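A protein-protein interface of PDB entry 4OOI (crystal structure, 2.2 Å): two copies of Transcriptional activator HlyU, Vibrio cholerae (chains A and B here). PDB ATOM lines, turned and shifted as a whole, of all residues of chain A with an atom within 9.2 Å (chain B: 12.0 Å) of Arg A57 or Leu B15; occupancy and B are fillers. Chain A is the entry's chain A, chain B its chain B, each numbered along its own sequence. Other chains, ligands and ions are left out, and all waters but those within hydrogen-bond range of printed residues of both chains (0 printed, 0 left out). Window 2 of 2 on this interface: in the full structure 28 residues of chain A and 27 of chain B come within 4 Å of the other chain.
Among the printed residues, merely in contact across the chains: Glu A35 with Ala B23, Glu A35 with Val B26, Gln A39 with Glu B19, Gln A39 with Ser B22, Cys A42 with Met B18, Arg A57 with Leu B15 and Leu A58 with Leu B15.
Arg A57 touches one residue of chain B.
Leu B15 touches just these residues of chain A: Arg A57 (3.2 Å) and Leu A58 (3.9 Å).
No residue of chain B comes within 4 Å of Glu A53.
No residue of chain B comes within 4 Å of Ser A56.
Leu A58 touches just one residue of chain B: Leu B15.
Glu A59 touches none of the printed residues of chain B.
No residue of chain A comes within 4 Å of Asn B14.
No residue of chain A comes within 4 Å of Gln B16.
Printed residues of chain A within 4 Å of Ala B23: Glu A35 (3.6 Å).
Printed residues of chain A within 4 Å of Ser B22: Gln A39 (3.5 Å).
Printed residues of chain B within 4 Å of Arg A36: Glu B19 (3.9 Å).
Leu A65 touches none of the printed residues of chain B.
The nearest residue of chain B that does not touch Arg A57 is Asn B14 (6.0 Å).
OE1 of Gln A39 sits at hydrogen-bond distance from NH1 of Arg A36, at 3.0 Å.
The guanidinium group (NH1) of Arg A36 sits at hydrogen-bond distance from the backbone carbonyl oxygen (O) of Leu A58 (3.3 Å).
The backbone carbonyl oxygen (O) of Met B18 lies within hydrogen-bond range of the side-chain hydroxyl (OG) of Ser B22, 3.0 Å away.
O of Glu B19 sits at hydrogen-bond distance from OG of Ser B22, at 3.1 Å.
No position is printed for both chains.
Printed residues of chain B that touch a printed residue of chain A: Leu B15, Met B18, Glu B19, Ser B22, Ala B23 and Val B26.
Hydrophobic or aromatic side chains of chain A within 4 Å of the printed part of chain B: Leu A58.
Among the printed residues, Asp or Glu carboxylates within 4 Å of a Lys or Arg side-chain nitrogen of the other chain: Arg A36 with Glu B19 (3.9 Å).
NH1 of Arg A36 is in salt-bridge range of OE2 of Glu B19, 3.9 Å away.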
ATOM      1  N   GLU A  35      10.564 -19.299 -25.480  1.00  0.00           N
ATOM      2  CA  GLU A  35       9.153 -19.478 -25.819  1.00  0.00           C
ATOM      3  C   GLU A  35       8.208 -19.173 -24.661  1.00  0.00           C
ATOM      4  O   GLU A  35       7.284 -18.372 -24.806  1.00  0.00           O
ATOM      5  CB  GLU A  35       8.897 -20.888 -26.362  1.00  0.00           C
ATOM      6  CG  GLU A  35       9.521 -21.139 -27.725  1.00  0.00           C
ATOM      7  CD  GLU A  35       9.097 -22.465 -28.326  1.00  0.00           C
ATOM      8  OE1 GLU A  35       8.373 -23.224 -27.646  1.00  0.00           O
ATOM      9  OE2 GLU A  35       9.487 -22.748 -29.478  1.00  0.00           O
ATOM     10  N   ARG A  36       8.447 -19.804 -23.517  1.00  0.00           N
ATOM     11  CA  ARG A  36       7.597 -19.602 -22.349  1.00  0.00           C
ATOM     12  C   ARG A  36       7.631 -18.155 -21.865  1.00  0.00           C
ATOM     13  O   ARG A  36       6.585 -17.552 -21.614  1.00  0.00           O
ATOM     14  CB  ARG A  36       7.994 -20.558 -21.221  1.00  0.00           C
ATOM     15  CG  ARG A  36       7.739 -22.023 -21.541  1.00  0.00           C
ATOM     16  CD  ARG A  36       6.332 -22.221 -22.080  1.00  0.00           C
ATOM     17  NE  ARG A  36       5.983 -23.632 -22.223  1.00  0.00           N
ATOM     18  CZ  ARG A  36       4.796 -24.067 -22.630  1.00  0.00           C
ATOM     19  NH1 ARG A  36       3.840 -23.200 -22.937  1.00  0.00           N
ATOM     20  NH2 ARG A  36       4.562 -25.368 -22.731  1.00  0.00           N
ATOM     21  N   GLN A  39       5.849 -15.911 -24.201  1.00  0.00           N
ATOM     22  CA  GLN A  39       4.410 -16.087 -24.036  1.00  0.00           C
ATOM     23  C   GLN A  39       3.900 -15.296 -22.834  1.00  0.00           C
ATOM     24  O   GLN A  39       2.863 -14.624 -22.908  1.00  0.00           O
ATOM     25  CB  GLN A  39       4.067 -17.569 -23.883  1.00  0.00           C
ATOM     26  CG  GLN A  39       4.178 -18.367 -25.173  1.00  0.00           C
ATOM     27  CD  GLN A  39       4.089 -19.864 -24.946  1.00  0.00           C
ATOM     28  OE1 GLN A  39       3.826 -20.321 -23.834  1.00  0.00           O
ATOM     29  NE2 GLN A  39       4.314 -20.635 -26.003  1.00  0.00           N
ATOM     30  N   ILE A  40       4.640 -15.380 -21.732  1.00  0.00           N
ATOM     31  CA  ILE A  40       4.325 -14.616 -20.531  1.00  0.00           C
ATOM     32  C   ILE A  40       4.275 -13.127 -20.845  1.00  0.00           C
ATOM     33  O   ILE A  40       3.299 -12.448 -20.524  1.00  0.00           O
ATOM     34  CB  ILE A  40       5.366 -14.849 -19.419  1.00  0.00           C
ATOM     35  CG1 ILE A  40       5.376 -16.316 -18.986  1.00  0.00           C
ATOM     36  CG2 ILE A  40       5.075 -13.953 -18.226  1.00  0.00           C
ATOM     37  CD1 ILE A  40       6.457 -16.647 -17.979  1.00  0.00           C
ATOM     38  N   CYS A  42       3.943 -11.670 -23.716  1.00  0.00           N
ATOM     39  CA  CYS A  42       2.877 -11.396 -24.673  1.00  0.00           C
ATOM     40  C   CYS A  42       1.523 -11.289 -23.986  1.00  0.00           C
ATOM     41  O   CYS A  42       0.696 -10.458 -24.359  1.00  0.00           O
ATOM     42  CB  CYS A  42       2.826 -12.474 -25.760  1.00  0.00           C
ATOM     43  SG  CYS A  42       4.083 -12.308 -27.047  1.00  0.00           S
ATOM     44  N   MET A  43       1.298 -12.130 -22.983  1.00  0.00           N
ATOM     45  CA  MET A  43       0.027 -12.107 -22.264  1.00  0.00           C
ATOM     46  C   MET A  43      -0.083 -10.949 -21.276  1.00  0.00           C
ATOM     47  O   MET A  43      -1.179 -10.605 -20.834  1.00  0.00           O
ATOM     48  CB  MET A  43      -0.217 -13.437 -21.553  1.00  0.00           C
ATOM     49  CG  MET A  43      -0.617 -14.555 -22.492  1.00  0.00           C
ATOM     50  SD  MET A  43      -1.061 -16.065 -21.623  1.00  0.00           S
ATOM     51  CE  MET A  43      -1.736 -17.027 -22.977  1.00  0.00           C
ATOM     52  N   LEU A  44       1.053 -10.350 -20.937  1.00  0.00           N
ATOM     53  CA  LEU A  44       1.078  -9.254 -19.972  1.00  0.00           C
ATOM     54  C   LEU A  44       0.984  -7.888 -20.646  1.00  0.00           C
ATOM     55  O   LEU A  44       0.944  -6.859 -19.973  1.00  0.00           O
ATOM     56  CB  LEU A  44       2.339  -9.327 -19.110  1.00  0.00           C
ATOM     57  CG  LEU A  44       2.427 -10.495 -18.128  1.00  0.00           C
ATOM     58  CD1 LEU A  44       3.748 -10.462 -17.378  1.00  0.00           C
ATOM     59  CD2 LEU A  44       1.258 -10.458 -17.162  1.00  0.00           C
ATOM     60  N   ASN A  47      -2.150  -5.586 -20.130  1.00  0.00           N
ATOM     61  CA  ASN A  47      -2.891  -6.446 -19.220  1.00  0.00           C
ATOM     62  C   ASN A  47      -2.155  -6.644 -17.902  1.00  0.00           C
ATOM     63  O   ASN A  47      -0.966  -6.347 -17.793  1.00  0.00           O
ATOM     64  CB  ASN A  47      -3.135  -7.807 -19.872  1.00  0.00           C
ATOM     65  CG  ASN A  47      -4.607  -8.139 -19.997  1.00  0.00           C
ATOM     66  OD1 ASN A  47      -5.450  -7.249 -20.109  1.00  0.00           O
ATOM     67  ND2 ASN A  47      -4.926  -9.428 -19.975  1.00  0.00           N
ATOM     68  N   GLU A  48      -2.872  -7.145 -16.903  1.00  0.00           N
ATOM     69  CA  GLU A  48      -2.269  -7.487 -15.624  1.00  0.00           C
ATOM     70  C   GLU A  48      -2.764  -8.858 -15.191  1.00  0.00           C
ATOM     71  O   GLU A  48      -3.955  -9.046 -14.939  1.00  0.00           O
ATOM     72  CB  GLU A  48      -2.611  -6.442 -14.564  1.00  0.00           C
ATOM     73  CG  GLU A  48      -1.916  -6.668 -13.231  1.00  0.00           C
ATOM     74  CD  GLU A  48      -2.201  -5.566 -12.231  1.00  0.00           C
ATOM     75  OE1 GLU A  48      -1.302  -5.246 -11.426  1.00  0.00           O
ATOM     76  OE2 GLU A  48      -3.326  -5.022 -12.248  1.00  0.00           O
ATOM     77  N   LEU A  49      -1.849  -9.816 -15.112  1.00  0.00           N
ATOM     78  CA  LEU A  49      -2.217 -11.194 -14.816  1.00  0.00           C
ATOM     79  C   LEU A  49      -1.519 -11.711 -13.565  1.00  0.00           C
ATOM     80  O   LEU A  49      -0.493 -11.176 -13.146  1.00  0.00           O
ATOM     81  CB  LEU A  49      -1.889 -12.098 -16.005  1.00  0.00           C
ATOM     82  CG  LEU A  49      -2.491 -11.691 -17.351  1.00  0.00           C
ATOM     83  CD1 LEU A  49      -2.043 -12.643 -18.448  1.00  0.00           C
ATOM     84  CD2 LEU A  49      -4.010 -11.638 -17.270  1.00  0.00           C
ATOM     85  N   SER A  50      -2.084 -12.759 -12.977  1.00  0.00           N
ATOM     86  CA  SER A  50      -1.502 -13.381 -11.796  1.00  0.00           C
ATOM     87  C   SER A  50      -0.745 -14.642 -12.184  1.00  0.00           C
ATOM     88  O   SER A  50      -0.806 -15.081 -13.332  1.00  0.00           O
ATOM     89  CB  SER A  50      -2.591 -13.721 -10.781  1.00  0.00           C
ATOM     90  OG  SER A  50      -3.503 -14.668 -11.308  1.00  0.00           O
ATOM     91  N   VAL A  51      -0.035 -15.221 -11.221  1.00  0.00           N
ATOM     92  CA  VAL A  51       0.735 -16.437 -11.461  1.00  0.00           C
ATOM     93  C   VAL A  51      -0.177 -17.597 -11.854  1.00  0.00           C
ATOM     94  O   VAL A  51       0.143 -18.369 -12.756  1.00  0.00           O
ATOM     95  CB  VAL A  51       1.564 -16.832 -10.224  1.00  0.00           C
ATOM     96  CG1 VAL A  51       2.374 -18.089 -10.502  1.00  0.00           C
ATOM     97  CG2 VAL A  51       2.477 -15.690  -9.813  1.00  0.00           C
ATOM     98  N   GLY A  52      -1.315 -17.707 -11.177  1.00  0.00           N
ATOM     99  CA  GLY A  52      -2.282 -18.747 -11.478  1.00  0.00           C
ATOM    100  C   GLY A  52      -2.874 -18.599 -12.866  1.00  0.00           C
ATOM    101  O   GLY A  52      -3.074 -19.586 -13.576  1.00  0.00           O
ATOM    102  N   GLU A  53      -3.155 -17.357 -13.251  1.00  0.00           N
ATOM    103  CA  GLU A  53      -3.717 -17.065 -14.566  1.00  0.00           C
ATOM    104  C   GLU A  53      -2.720 -17.377 -15.676  1.00  0.00           C
ATOM    105  O   GLU A  53      -3.087 -17.930 -16.713  1.00  0.00           O
ATOM    106  CB  GLU A  53      -4.162 -15.603 -14.646  1.00  0.00           C
ATOM    107  CG  GLU A  53      -5.395 -15.289 -13.813  1.00  0.00           C
ATOM    108  CD  GLU A  53      -5.644 -13.799 -13.673  1.00  0.00           C
ATOM    109  OE1 GLU A  53      -4.686 -13.018 -13.843  1.00  0.00           O
ATOM    110  OE2 GLU A  53      -6.798 -13.411 -13.395  1.00  0.00           O
ATOM    111  N   LEU A  54      -1.459 -17.017 -15.454  1.00  0.00           N
ATOM    112  CA  LEU A  54      -0.397 -17.315 -16.407  1.00  0.00           C
ATOM    113  C   LEU A  54      -0.205 -18.821 -16.537  1.00  0.00           C
ATOM    114  O   LEU A  54      -0.093 -19.348 -17.643  1.00  0.00           O
ATOM    115  CB  LEU A  54       0.915 -16.662 -15.969  1.00  0.00           C
ATOM    116  CG  LEU A  54       0.989 -15.135 -16.031  1.00  0.00           C
ATOM    117  CD1 LEU A  54       2.281 -14.638 -15.402  1.00  0.00           C
ATOM    118  CD2 LEU A  54       0.875 -14.658 -17.469  1.00  0.00           C
ATOM    119  N   SER A  55      -0.174 -19.505 -15.399  1.00  0.00           N
ATOM    120  CA  SER A  55       0.014 -20.951 -15.364  1.00  0.00           C
ATOM    121  C   SER A  55      -1.152 -21.684 -16.015  1.00  0.00           C
ATOM    122  O   SER A  55      -0.986 -22.778 -16.553  1.00  0.00           O
ATOM    123  CB  SER A  55       0.188 -21.429 -13.921  1.00  0.00           C
ATOM    124  OG  SER A  55       0.179 -22.844 -13.849  1.00  0.00           O
ATOM    125  N   SER A  56      -2.332 -21.078 -15.962  1.00  0.00           N
ATOM    126  CA  SER A  56      -3.523 -21.685 -16.540  1.00  0.00           C
ATOM    127  C   SER A  56      -3.599 -21.452 -18.044  1.00  0.00           C
ATOM    128  O   SER A  56      -3.916 -22.366 -18.806  1.00  0.00           O
ATOM    129  CB  SER A  56      -4.781 -21.146 -15.859  1.00  0.00           C
ATOM    130  OG  SER A  56      -5.953 -21.623 -16.496  1.00  0.00           O
ATOM    131  N   ARG A  57      -3.304 -20.227 -18.468  1.00  0.00           N
ATOM    132  CA  ARG A  57      -3.375 -19.874 -19.880  1.00  0.00           C
ATOM    133  C   ARG A  57      -2.201 -20.426 -20.684  1.00  0.00           C
ATOM    134  O   ARG A  57      -2.293 -20.570 -21.900  1.00  0.00           O
ATOM    135  CB  ARG A  57      -3.467 -18.357 -20.061  1.00  0.00           C
ATOM    136  CG  ARG A  57      -4.783 -17.753 -19.601  1.00  0.00           C
ATOM    137  CD  ARG A  57      -4.964 -16.346 -20.147  1.00  0.00           C
ATOM    138  NE  ARG A  57      -6.259 -15.780 -19.780  1.00  0.00           N
ATOM    139  CZ  ARG A  57      -7.386 -15.992 -20.453  1.00  0.00           C
ATOM    140  NH1 ARG A  57      -7.381 -16.761 -21.533  1.00  0.00           N
ATOM    141  NH2 ARG A  57      -8.518 -15.436 -20.045  1.00  0.00           N
ATOM    142  N   LEU A  58      -1.100 -20.732 -20.005  1.00  0.00           N
ATOM    143  CA  LEU A  58       0.082 -21.262 -20.678  1.00  0.00           C
ATOM    144  C   LEU A  58       0.260 -22.753 -20.421  1.00  0.00           C
ATOM    145  O   LEU A  58       1.126 -23.393 -21.019  1.00  0.00           O
ATOM    146  CB  LEU A  58       1.337 -20.505 -20.240  1.00  0.00           C
ATOM    147  CG  LEU A  58       1.387 -19.029 -20.631  1.00  0.00           C
ATOM    148  CD1 LEU A  58       2.670 -18.388 -20.138  1.00  0.00           C
ATOM    149  CD2 LEU A  58       1.256 -18.883 -22.136  1.00  0.00           C
ATOM    150  N   GLU A  59      -0.571 -23.292 -19.532  1.00  0.00           N
ATOM    151  CA  GLU A  59      -0.503 -24.699 -19.141  1.00  0.00           C
ATOM    152  C   GLU A  59       0.883 -25.086 -18.631  1.00  0.00           C
ATOM    153  O   GLU A  59       1.548 -25.948 -19.205  1.00  0.00           O
ATOM    154  CB  GLU A  59      -0.934 -25.610 -20.293  1.00  0.00           C
ATOM    155  CG  GLU A  59      -2.365 -25.387 -20.753  1.00  0.00           C
ATOM    156  CD  GLU A  59      -2.782 -26.344 -21.850  1.00  0.00           C
ATOM    157  OE1 GLU A  59      -1.931 -27.140 -22.299  1.00  0.00           O
ATOM    158  OE2 GLU A  59      -3.960 -26.303 -22.261  1.00  0.00           O
ATOM    159  N   LEU A  60       1.308 -24.435 -17.554  1.00  0.00           N
ATOM    160  CA  LEU A  60       2.586 -24.731 -16.919  1.00  0.00           C
ATOM    161  C   LEU A  60       2.411 -24.887 -15.414  1.00  0.00           C
ATOM    162  O   LEU A  60       1.459 -24.366 -14.835  1.00  0.00           O
ATOM    163  CB  LEU A  60       3.592 -23.613 -17.195  1.00  0.00           C
ATOM    164  CG  LEU A  60       4.260 -23.568 -18.568  1.00  0.00           C
ATOM    165  CD1 LEU A  60       5.075 -22.293 -18.707  1.00  0.00           C
ATOM    166  CD2 LEU A  60       5.141 -24.790 -18.765  1.00  0.00           C
ATOM    167  N   LEU A  65       6.951 -22.072 -14.176  1.00  0.00           N
ATOM    168  CA  LEU A  65       6.567 -20.697 -14.449  1.00  0.00           C
ATOM    169  C   LEU A  65       7.365 -19.745 -13.563  1.00  0.00           C
ATOM    170  O   LEU A  65       7.742 -18.656 -13.993  1.00  0.00           O
ATOM    171  CB  LEU A  65       5.068 -20.511 -14.204  1.00  0.00           C
ATOM    172  CG  LEU A  65       4.442 -19.187 -14.641  1.00  0.00           C
ATOM    173  CD1 LEU A  65       4.398 -19.083 -16.157  1.00  0.00           C
ATOM    174  CD2 LEU A  65       3.051 -19.040 -14.053  1.00  0.00           C
ATOM    175  N   CYS A 108       0.830 -12.179 -34.395  1.00  0.00           N
ATOM    176  CA  CYS A 108      -0.396 -12.597 -33.714  1.00  0.00           C
ATOM    177  C   CYS A 108      -1.697 -12.134 -34.369  1.00  0.00           C
ATOM    178  O   CYS A 108      -2.784 -12.472 -33.898  1.00  0.00           O
ATOM    179  CB  CYS A 108      -0.365 -12.178 -32.239  1.00  0.00           C
ATOM    180  SG  CYS A 108       0.876 -13.043 -31.244  1.00  0.00           S
ATOM    181  N   ASN B  14      -6.660 -20.763 -29.686  1.00  0.00           N
ATOM    182  CA  ASN B  14      -5.867 -19.545 -29.566  1.00  0.00           C
ATOM    183  C   ASN B  14      -4.429 -19.804 -29.120  1.00  0.00           C
ATOM    184  O   ASN B  14      -3.483 -19.426 -29.810  1.00  0.00           O
ATOM    185  CB  ASN B  14      -6.546 -18.550 -28.620  1.00  0.00           C
ATOM    186  CG  ASN B  14      -5.602 -17.465 -28.136  1.00  0.00           C
ATOM    187  OD1 ASN B  14      -5.039 -17.561 -27.045  1.00  0.00           O
ATOM    188  ND2 ASN B  14      -5.423 -16.427 -28.944  1.00  0.00           N
ATOM    189  N   LEU B  15      -4.275 -20.451 -27.968  1.00  0.00           N
ATOM    190  CA  LEU B  15      -2.959 -20.688 -27.375  1.00  0.00           C
ATOM    191  C   LEU B  15      -2.037 -21.511 -28.270  1.00  0.00           C
ATOM    192  O   LEU B  15      -0.844 -21.231 -28.369  1.00  0.00           O
ATOM    193  CB  LEU B  15      -3.096 -21.377 -26.015  1.00  0.00           C
ATOM    194  CG  LEU B  15      -1.785 -21.770 -25.329  1.00  0.00           C
ATOM    195  CD1 LEU B  15      -1.029 -20.536 -24.851  1.00  0.00           C
ATOM    196  CD2 LEU B  15      -2.036 -22.738 -24.182  1.00  0.00           C
ATOM    197  N   GLN B  16      -2.596 -22.531 -28.910  1.00  0.00           N
ATOM    198  CA  GLN B  16      -1.814 -23.407 -29.773  1.00  0.00           C
ATOM    199  C   GLN B  16      -1.234 -22.633 -30.959  1.00  0.00           C
ATOM    200  O   GLN B  16      -0.076 -22.832 -31.336  1.00  0.00           O
ATOM    201  CB  GLN B  16      -2.667 -24.587 -30.239  1.00  0.00           C
ATOM    202  CG  GLN B  16      -3.431 -25.265 -29.103  1.00  0.00           C
ATOM    203  CD  GLN B  16      -2.521 -25.736 -27.982  1.00  0.00           C
ATOM    204  OE1 GLN B  16      -1.480 -26.347 -28.225  1.00  0.00           O
ATOM    205  NE2 GLN B  16      -2.908 -25.447 -26.744  1.00  0.00           N
ATOM    206  N   GLU B  17      -2.032 -21.735 -31.532  1.00  0.00           N
ATOM    207  CA  GLU B  17      -1.542 -20.854 -32.589  1.00  0.00           C
ATOM    208  C   GLU B  17      -0.515 -19.864 -32.039  1.00  0.00           C
ATOM    209  O   GLU B  17       0.465 -19.525 -32.715  1.00  0.00           O
ATOM    210  CB  GLU B  17      -2.698 -20.113 -33.267  1.00  0.00           C
ATOM    211  CG  GLU B  17      -3.560 -20.986 -34.171  1.00  0.00           C
ATOM    212  CD  GLU B  17      -4.618 -21.762 -33.413  1.00  0.00           C
ATOM    213  OE1 GLU B  17      -5.129 -21.240 -32.399  1.00  0.00           O
ATOM    214  OE2 GLU B  17      -4.941 -22.894 -33.831  1.00  0.00           O
ATOM    215  N   MET B  18      -0.742 -19.405 -30.810  1.00  0.00           N
ATOM    216  CA  MET B  18       0.210 -18.530 -30.131  1.00  0.00           C
ATOM    217  C   MET B  18       1.581 -19.195 -30.026  1.00  0.00           C
ATOM    218  O   MET B  18       2.603 -18.542 -30.208  1.00  0.00           O
ATOM    219  CB  MET B  18      -0.309 -18.117 -28.747  1.00  0.00           C
ATOM    220  CG  MET B  18       0.779 -17.943 -27.692  1.00  0.00           C
ATOM    221  SD  MET B  18       0.373 -16.741 -26.411  1.00  0.00           S
ATOM    222  CE  MET B  18       0.559 -15.207 -27.318  1.00  0.00           C
ATOM    223  N   GLU B  19       1.590 -20.497 -29.746  1.00  0.00           N
ATOM    224  CA  GLU B  19       2.824 -21.276 -29.729  1.00  0.00           C
ATOM    225  C   GLU B  19       3.383 -21.403 -31.145  1.00  0.00           C
ATOM    226  O   GLU B  19       4.594 -21.263 -31.367  1.00  0.00           O
ATOM    227  CB  GLU B  19       2.570 -22.666 -29.131  1.00  0.00           C
ATOM    228  CG  GLU B  19       2.098 -22.655 -27.677  1.00  0.00           C
ATOM    229  CD  GLU B  19       1.785 -24.043 -27.144  1.00  0.00           C
ATOM    230  OE1 GLU B  19       1.798 -25.005 -27.939  1.00  0.00           O
ATOM    231  OE2 GLU B  19       1.526 -24.172 -25.927  1.00  0.00           O
ATOM    232  N   LYS B  20       2.483 -21.655 -32.095  1.00  0.00           N
ATOM    233  CA  LYS B  20       2.831 -21.791 -33.511  1.00  0.00           C
ATOM    234  C   LYS B  20       3.620 -20.590 -34.037  1.00  0.00           C
ATOM    235  O   LYS B  20       4.533 -20.749 -34.849  1.00  0.00           O
ATOM    236  CB  LYS B  20       1.564 -22.042 -34.350  1.00  0.00           C
ATOM    237  CG  LYS B  20       1.346 -21.092 -35.528  1.00  0.00           C
ATOM    238  CD  LYS B  20      -0.085 -21.176 -36.066  1.00  0.00           C
ATOM    239  CE  LYS B  20      -0.595 -19.800 -36.497  1.00  0.00           C
ATOM    240  NZ  LYS B  20      -1.986 -19.825 -37.041  1.00  0.00           N
ATOM    241  N   ASN B  21       3.284 -19.394 -33.558  1.00  0.00           N
ATOM    242  CA  ASN B  21       4.003 -18.188 -33.974  1.00  0.00           C
ATOM    243  C   ASN B  21       5.155 -17.782 -33.055  1.00  0.00           C
ATOM    244  O   ASN B  21       6.182 -17.271 -33.514  1.00  0.00           O
ATOM    245  CB  ASN B  21       3.038 -17.016 -34.139  1.00  0.00           C
ATOM    246  CG  ASN B  21       2.256 -17.086 -35.432  1.00  0.00           C
ATOM    247  OD1 ASN B  21       1.027 -17.142 -35.424  1.00  0.00           O
ATOM    248  ND2 ASN B  21       2.966 -17.083 -36.554  1.00  0.00           N
ATOM    249  N   SER B  22       4.980 -18.011 -31.757  1.00  0.00           N
ATOM    250  CA  SER B  22       6.010 -17.683 -30.783  1.00  0.00           C
ATOM    251  C   SER B  22       7.244 -18.537 -31.015  1.00  0.00           C
ATOM    252  O   SER B  22       8.338 -18.164 -30.612  1.00  0.00           O
ATOM    253  CB  SER B  22       5.506 -17.880 -29.355  1.00  0.00           C
ATOM    254  OG  SER B  22       5.268 -19.251 -29.087  1.00  0.00           O
ATOM    255  N   ALA B  23       7.064 -19.690 -31.654  1.00  0.00           N
ATOM    256  CA  ALA B  23       8.200 -20.517 -32.043  1.00  0.00           C
ATOM    257  C   ALA B  23       9.100 -19.752 -33.014  1.00  0.00           C
ATOM    258  O   ALA B  23      10.308 -19.625 -32.792  1.00  0.00           O
ATOM    259  CB  ALA B  23       7.718 -21.814 -32.671  1.00  0.00           C
ATOM    260  N   LYS B  24       8.496 -19.237 -34.082  1.00  0.00           N
ATOM    261  CA  LYS B  24       9.213 -18.447 -35.077  1.00  0.00           C
ATOM    262  C   LYS B  24       9.828 -17.209 -34.439  1.00  0.00           C
ATOM    263  O   LYS B  24      11.016 -16.913 -34.631  1.00  0.00           O
ATOM    264  CB  LYS B  24       8.267 -18.015 -36.200  1.00  0.00           C
ATOM    265  CG  LYS B  24       7.494 -19.144 -36.861  1.00  0.00           C
ATOM    266  CD  LYS B  24       6.641 -18.618 -38.006  1.00  0.00           C
ATOM    267  CE  LYS B  24       5.796 -19.719 -38.629  1.00  0.00           C
ATOM    268  NZ  LYS B  24       4.818 -20.290 -37.661  1.00  0.00           N
ATOM    269  N   ALA B  25       9.006 -16.489 -33.677  1.00  0.00           N
ATOM    270  CA  ALA B  25       9.443 -15.270 -33.003  1.00  0.00           C
ATOM    271  C   ALA B  25      10.650 -15.532 -32.109  1.00  0.00           C
ATOM    272  O   ALA B  25      11.556 -14.704 -32.011  1.00  0.00           O
ATOM    273  CB  ALA B  25       8.301 -14.676 -32.194  1.00  0.00           C
ATOM    274  N   VAL B  26      10.657 -16.694 -31.465  1.00  0.00           N
ATOM    275  CA  VAL B  26      11.756 -17.088 -30.591  1.00  0.00           C
ATOM    276  C   VAL B  26      12.985 -17.495 -31.401  1.00  0.00           C
ATOM    277  O   VAL B  26      14.111 -17.289 -30.962  1.00  0.00           O
ATOM    278  CB  VAL B  26      11.325 -18.197 -29.595  1.00  0.00           C
ATOM    279  CG1 VAL B  26      12.524 -18.939 -29.025  1.00  0.00           C
ATOM    280  CG2 VAL B  26      10.508 -17.587 -28.475  1.00  0.00           C
